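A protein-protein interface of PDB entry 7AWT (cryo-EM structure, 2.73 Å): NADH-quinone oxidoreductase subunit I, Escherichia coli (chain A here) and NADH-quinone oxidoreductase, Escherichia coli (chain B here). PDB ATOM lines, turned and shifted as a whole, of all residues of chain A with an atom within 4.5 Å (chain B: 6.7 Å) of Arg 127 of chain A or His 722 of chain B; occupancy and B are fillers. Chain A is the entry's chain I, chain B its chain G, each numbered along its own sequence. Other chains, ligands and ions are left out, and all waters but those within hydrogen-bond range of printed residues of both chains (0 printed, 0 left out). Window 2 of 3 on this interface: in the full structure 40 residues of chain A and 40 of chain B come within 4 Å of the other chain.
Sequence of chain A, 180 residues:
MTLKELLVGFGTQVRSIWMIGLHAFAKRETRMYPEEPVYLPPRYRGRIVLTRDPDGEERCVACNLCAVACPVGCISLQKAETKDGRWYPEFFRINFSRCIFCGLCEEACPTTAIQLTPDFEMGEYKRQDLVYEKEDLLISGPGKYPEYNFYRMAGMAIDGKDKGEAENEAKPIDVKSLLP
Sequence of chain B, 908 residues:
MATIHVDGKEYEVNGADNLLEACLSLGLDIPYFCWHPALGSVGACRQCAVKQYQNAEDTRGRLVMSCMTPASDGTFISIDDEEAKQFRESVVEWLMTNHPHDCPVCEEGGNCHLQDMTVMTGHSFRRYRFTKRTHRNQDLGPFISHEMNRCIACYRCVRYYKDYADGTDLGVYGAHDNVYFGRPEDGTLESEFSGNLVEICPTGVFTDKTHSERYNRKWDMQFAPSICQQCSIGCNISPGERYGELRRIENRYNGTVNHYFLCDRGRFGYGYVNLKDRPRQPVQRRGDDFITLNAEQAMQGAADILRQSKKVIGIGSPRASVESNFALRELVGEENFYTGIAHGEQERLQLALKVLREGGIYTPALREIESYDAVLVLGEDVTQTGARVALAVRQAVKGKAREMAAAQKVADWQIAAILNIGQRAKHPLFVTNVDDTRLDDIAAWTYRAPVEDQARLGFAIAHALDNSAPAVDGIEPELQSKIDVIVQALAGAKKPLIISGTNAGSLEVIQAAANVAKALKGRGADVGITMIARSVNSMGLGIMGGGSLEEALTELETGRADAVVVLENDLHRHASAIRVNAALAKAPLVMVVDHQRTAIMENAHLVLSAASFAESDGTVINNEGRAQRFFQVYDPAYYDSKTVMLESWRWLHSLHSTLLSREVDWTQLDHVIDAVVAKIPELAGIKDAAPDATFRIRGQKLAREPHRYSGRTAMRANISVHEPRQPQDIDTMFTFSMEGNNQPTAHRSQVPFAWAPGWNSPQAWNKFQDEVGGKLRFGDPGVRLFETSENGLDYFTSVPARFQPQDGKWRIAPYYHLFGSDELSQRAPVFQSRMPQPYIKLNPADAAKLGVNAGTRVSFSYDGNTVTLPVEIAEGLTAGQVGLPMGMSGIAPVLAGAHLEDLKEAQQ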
ATOM      1  N   SER A  97      20.704 -24.661  -1.432  1.00  0.00           N
ATOM      2  CA  SER A  97      21.055 -26.062  -1.451  1.00  0.00           C
ATOM      3  C   SER A  97      22.530 -26.190  -1.087  1.00  0.00           C
ATOM      4  O   SER A  97      23.006 -27.278  -0.896  1.00  0.00           O
ATOM      5  CB  SER A  97      20.756 -26.703  -2.786  1.00  0.00           C
ATOM      6  OG  SER A  97      21.254 -25.933  -3.837  1.00  0.00           O
ATOM      7  N   TYR A 125      10.855 -29.462  -3.556  1.00  0.00           N
ATOM      8  CA  TYR A 125      10.727 -30.707  -4.297  1.00  0.00           C
ATOM      9  C   TYR A 125      11.773 -30.867  -5.389  1.00  0.00           C
ATOM     10  O   TYR A 125      12.115 -32.004  -5.731  1.00  0.00           O
ATOM     11  CB  TYR A 125       9.342 -30.803  -4.949  1.00  0.00           C
ATOM     12  CG  TYR A 125       8.232 -31.283  -4.048  1.00  0.00           C
ATOM     13  CD1 TYR A 125       7.986 -32.637  -3.880  1.00  0.00           C
ATOM     14  CD2 TYR A 125       7.418 -30.383  -3.380  1.00  0.00           C
ATOM     15  CE1 TYR A 125       6.968 -33.080  -3.065  1.00  0.00           C
ATOM     16  CE2 TYR A 125       6.395 -30.815  -2.566  1.00  0.00           C
ATOM     17  CZ  TYR A 125       6.177 -32.164  -2.409  1.00  0.00           C
ATOM     18  OH  TYR A 125       5.159 -32.599  -1.593  1.00  0.00           O
ATOM     19  N   LYS A 126      12.281 -29.771  -5.951  1.00  0.00           N
ATOM     20  CA  LYS A 126      13.079 -29.841  -7.162  1.00  0.00           C
ATOM     21  C   LYS A 126      14.512 -29.356  -7.008  1.00  0.00           C
ATOM     22  O   LYS A 126      15.310 -29.564  -7.928  1.00  0.00           O
ATOM     23  CB  LYS A 126      12.408 -29.033  -8.283  1.00  0.00           C
ATOM     24  CG  LYS A 126      10.909 -29.247  -8.385  1.00  0.00           C
ATOM     25  CD  LYS A 126      10.576 -30.646  -8.871  1.00  0.00           C
ATOM     26  CE  LYS A 126      10.449 -30.686 -10.383  1.00  0.00           C
ATOM     27  NZ  LYS A 126      11.206 -31.823 -10.975  1.00  0.00           N
ATOM     28  N   ARG A 127      14.807 -28.633  -5.950  1.00  0.00           N
ATOM     29  CA  ARG A 127      16.161 -28.189  -5.664  1.00  0.00           C
ATOM     30  C   ARG A 127      16.478 -26.954  -6.446  1.00  0.00           C
ATOM     31  O   ARG A 127      17.360 -26.199  -6.102  1.00  0.00           O
ATOM     32  CB  ARG A 127      17.196 -29.257  -5.951  1.00  0.00           C
ATOM     33  CG  ARG A 127      18.529 -28.936  -5.309  1.00  0.00           C
ATOM     34  CD  ARG A 127      19.567 -29.982  -5.606  1.00  0.00           C
ATOM     35  NE  ARG A 127      20.856 -29.373  -5.844  1.00  0.00           N
ATOM     36  CZ  ARG A 127      21.875 -29.992  -6.410  1.00  0.00           C
ATOM     37  NH1 ARG A 127      21.762 -31.250  -6.784  1.00  0.00           N
ATOM     38  NH2 ARG A 127      23.013 -29.349  -6.593  1.00  0.00           N
ATOM     39  N   GLN A 128      15.772 -26.785  -7.547  1.00  0.00           N
ATOM     40  CA  GLN A 128      15.825 -25.556  -8.294  1.00  0.00           C
ATOM     41  C   GLN A 128      15.071 -24.482  -7.511  1.00  0.00           C
ATOM     42  O   GLN A 128      15.466 -23.343  -7.509  1.00  0.00           O
ATOM     43  CB  GLN A 128      15.261 -25.737  -9.683  1.00  0.00           C
ATOM     44  CG  GLN A 128      15.128 -24.445 -10.436  1.00  0.00           C
ATOM     45  CD  GLN A 128      16.411 -23.667 -10.458  1.00  0.00           C
ATOM     46  OE1 GLN A 128      17.425 -24.163 -10.903  1.00  0.00           O
ATOM     47  NE2 GLN A 128      16.366 -22.437  -9.991  1.00  0.00           N
ATOM     48  N   ASP A 129      13.959 -24.846  -6.876  1.00  0.00           N
ATOM     49  CA  ASP A 129      13.136 -23.938  -6.098  1.00  0.00           C
ATOM     50  C   ASP A 129      13.769 -23.591  -4.759  1.00  0.00           C
ATOM     51  O   ASP A 129      13.139 -22.901  -3.954  1.00  0.00           O
ATOM     52  CB  ASP A 129      11.753 -24.553  -5.886  1.00  0.00           C
ATOM     53  CG  ASP A 129      10.993 -24.740  -7.182  1.00  0.00           C
ATOM     54  OD1 ASP A 129      11.518 -24.349  -8.246  1.00  0.00           O
ATOM     55  OD2 ASP A 129       9.872 -25.283  -7.141  1.00  0.00           O
ATOM     56  N   LEU A 130      14.985 -24.065  -4.503  1.00  0.00           N
ATOM     57  CA  LEU A 130      15.752 -23.705  -3.319  1.00  0.00           C
ATOM     58  C   LEU A 130      16.718 -22.564  -3.590  1.00  0.00           C
ATOM     59  O   LEU A 130      17.593 -22.297  -2.763  1.00  0.00           O
ATOM     60  CB  LEU A 130      16.517 -24.921  -2.793  1.00  0.00           C
ATOM     61  CG  LEU A 130      15.820 -25.814  -1.771  1.00  0.00           C
ATOM     62  CD1 LEU A 130      16.626 -27.071  -1.522  1.00  0.00           C
ATOM     63  CD2 LEU A 130      15.603 -25.062  -0.480  1.00  0.00           C
ATOM     64  N   VAL A 131      16.587 -21.899  -4.728  1.00  0.00           N
ATOM     65  CA  VAL A 131      17.409 -20.750  -5.082  1.00  0.00           C
ATOM     66  C   VAL A 131      16.533 -19.514  -4.947  1.00  0.00           C
ATOM     67  O   VAL A 131      15.654 -19.271  -5.781  1.00  0.00           O
ATOM     68  CB  VAL A 131      17.976 -20.877  -6.500  1.00  0.00           C
ATOM     69  CG1 VAL A 131      18.919 -19.738  -6.789  1.00  0.00           C
ATOM     70  CG2 VAL A 131      18.681 -22.206  -6.666  1.00  0.00           C
ATOM     71  N   ARG B 716      25.398 -19.025 -11.449  1.00  0.00           N
ATOM     72  CA  ARG B 716      24.701 -19.648 -12.567  1.00  0.00           C
ATOM     73  C   ARG B 716      23.542 -20.505 -12.075  1.00  0.00           C
ATOM     74  O   ARG B 716      23.197 -21.510 -12.693  1.00  0.00           O
ATOM     75  CB  ARG B 716      25.664 -20.478 -13.412  1.00  0.00           C
ATOM     76  CG  ARG B 716      25.309 -20.532 -14.884  1.00  0.00           C
ATOM     77  CD  ARG B 716      26.148 -21.561 -15.612  1.00  0.00           C
ATOM     78  NE  ARG B 716      25.438 -22.825 -15.774  1.00  0.00           N
ATOM     79  CZ  ARG B 716      24.740 -23.155 -16.855  1.00  0.00           C
ATOM     80  NH1 ARG B 716      24.127 -24.328 -16.919  1.00  0.00           N
ATOM     81  NH2 ARG B 716      24.656 -22.312 -17.876  1.00  0.00           N
ATOM     82  N   ALA B 717      22.935 -20.115 -10.956  1.00  0.00           N
ATOM     83  CA  ALA B 717      21.891 -20.916 -10.336  1.00  0.00           C
ATOM     84  C   ALA B 717      20.514 -20.666 -10.930  1.00  0.00           C
ATOM     85  O   ALA B 717      19.669 -21.566 -10.906  1.00  0.00           O
ATOM     86  CB  ALA B 717      21.848 -20.652  -8.830  1.00  0.00           C
ATOM     87  N   SER B 720      20.400 -23.112 -13.954  1.00  0.00           N
ATOM     88  CA  SER B 720      20.312 -24.475 -13.453  1.00  0.00           C
ATOM     89  C   SER B 720      21.131 -24.566 -12.178  1.00  0.00           C
ATOM     90  O   SER B 720      22.249 -24.055 -12.101  1.00  0.00           O
ATOM     91  CB  SER B 720      20.803 -25.492 -14.485  1.00  0.00           C
ATOM     92  OG  SER B 720      20.752 -26.807 -13.964  1.00  0.00           O
ATOM     93  N   VAL B 721      20.565 -25.239 -11.177  1.00  0.00           N
ATOM     94  CA  VAL B 721      21.202 -25.292  -9.867  1.00  0.00           C
ATOM     95  C   VAL B 721      22.413 -26.220  -9.854  1.00  0.00           C
ATOM     96  O   VAL B 721      23.304 -26.050  -9.010  1.00  0.00           O
ATOM     97  CB  VAL B 721      20.176 -25.710  -8.798  1.00  0.00           C
ATOM     98  CG1 VAL B 721      19.582 -27.067  -9.129  1.00  0.00           C
ATOM     99  CG2 VAL B 721      20.780 -25.684  -7.406  1.00  0.00           C
ATOM    100  N   HIS B 722      22.492 -27.168 -10.783  1.00  0.00           N
ATOM    101  CA  HIS B 722      23.664 -28.031 -10.905  1.00  0.00           C
ATOM    102  C   HIS B 722      24.744 -27.261 -11.650  1.00  0.00           C
ATOM    103  O   HIS B 722      24.680 -27.104 -12.870  1.00  0.00           O
ATOM    104  CB  HIS B 722      23.309 -29.324 -11.627  1.00  0.00           C
ATOM    105  CG  HIS B 722      22.065 -29.978 -11.114  1.00  0.00           C
ATOM    106  ND1 HIS B 722      22.059 -30.790 -10.003  1.00  0.00           N
ATOM    107  CD2 HIS B 722      20.788 -29.937 -11.560  1.00  0.00           C
ATOM    108  CE1 HIS B 722      20.829 -31.223  -9.786  1.00  0.00           C
ATOM    109  NE2 HIS B 722      20.039 -30.721 -10.716  1.00  0.00           N
ATOM    110  N   GLU B 723      25.740 -26.778 -10.915  1.00  0.00           N
ATOM    111  CA  GLU B 723      26.780 -25.964 -11.520  1.00  0.00           C
ATOM    112  C   GLU B 723      27.552 -26.780 -12.556  1.00  0.00           C
ATOM    113  O   GLU B 723      27.829 -27.963 -12.335  1.00  0.00           O
ATOM    114  CB  GLU B 723      27.741 -25.432 -10.457  1.00  0.00           C
ATOM    115  CG  GLU B 723      28.083 -26.434  -9.376  1.00  0.00           C
ATOM    116  CD  GLU B 723      27.144 -26.355  -8.195  1.00  0.00           C
ATOM    117  OE1 GLU B 723      27.506 -26.855  -7.113  1.00  0.00           O
ATOM    118  OE2 GLU B 723      26.045 -25.785  -8.344  1.00  0.00           O
ATOM    119  N   PRO B 724      27.909 -26.186 -13.686  1.00  0.00           N
ATOM    120  CA  PRO B 724      28.643 -26.922 -14.716  1.00  0.00           C
ATOM    121  C   PRO B 724      30.120 -27.025 -14.366  1.00  0.00           C
ATOM    122  O   PRO B 724      30.608 -26.426 -13.410  1.00  0.00           O
ATOM    123  CB  PRO B 724      28.430 -26.068 -15.965  1.00  0.00           C
ATOM    124  CG  PRO B 724      28.325 -24.679 -15.426  1.00  0.00           C
ATOM    125  CD  PRO B 724      27.664 -24.786 -14.075  1.00  0.00           C
ATOM    126  N   ARG B 725      30.832 -27.809 -15.168  1.00  0.00           N
ATOM    127  CA  ARG B 725      32.277 -27.877 -15.032  1.00  0.00           C
ATOM    128  C   ARG B 725      32.904 -26.588 -15.544  1.00  0.00           C
ATOM    129  O   ARG B 725      32.393 -25.948 -16.466  1.00  0.00           O
ATOM    130  CB  ARG B 725      32.833 -29.072 -15.803  1.00  0.00           C
ATOM    131  CG  ARG B 725      32.466 -29.084 -17.275  1.00  0.00           C
ATOM    132  CD  ARG B 725      32.996 -30.328 -17.972  1.00  0.00           C
ATOM    133  NE  ARG B 725      34.425 -30.239 -18.266  1.00  0.00           N
ATOM    134  CZ  ARG B 725      35.382 -30.760 -17.505  1.00  0.00           C
ATOM    135  NH1 ARG B 725      35.072 -31.408 -16.393  1.00  0.00           N
ATOM    136  NH2 ARG B 725      36.652 -30.633 -17.856  1.00  0.00           N
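The side-chain amide oxygen of Gln 128 of chain A lies close to the backbone carbonyl oxygen of Ala 717 of chain B (3.4 Å).
OE1 of Gln 128 of chain A lies within hydrogen-bond range of N of Val 721 of chain B.
NH1 of Arg 127 of chain A lies close to ND1 of His 722 of chain B, at 3.3 Å.
CG2 of Val 721 of chain B touches OG of Ser 97 of chain A, 3.6 Å away.
O of Arg 127 of chain A touches CG2 of Val 721 of chain B (3.7 Å).
Ser 720 of chain B touches Gln 128 of chain A (CA to OE1, 3.9 Å).
Val 131 of chain A touches Ala 717 of chain B.
Arg 127 of chain A touches just these residues of chain B: Val 721 and His 722.
His 722 of chain B touches just one residue of chain A: Arg 127 (3.1 Å).
Of the printed residues of chain A, Ser 720 of chain B touches Gln 128 (3.9 Å).
Printed residues of chain B within 4 Å of Gln 128 of chain A: Ala 717, Ser 720 and Val 721.
Of the printed residues of chain A, Val 721 of chain B touches Ser 97 (3.6 Å), Arg 127 (3.7 Å) and Gln 128 (3.3 Å).
Of the printed residues of chain A, Ala 717 of chain B touches Gln 128 (3.4 Å) and Val 131 (3.7 Å).
Glu 723 of chain B touches none of the printed residues of chain A.
The nearest printed residue of chain A that does not touch Ala 717 of chain B is Arg 127 of chain A (7.1 Å).
Of the 8 printed residues of chain A, 4 touch a printed residue of chain B.
Along chain A the printed residues that touch a printed residue of chain B span positions 97 to 131.
Of the 8 printed residues of chain B, 4 touch a printed residue of chain A.
Hydrophobic or aromatic side chains of chain B that line the printed part of chain A: Ala 717, Val 721 and His 722.
Among the printed residues, 7 pairs touch across the chains.
Among the printed residues, no Asp or Glu carboxylate lies within 4 Å of a Lys or Arg side-chain nitrogen of the other chain.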
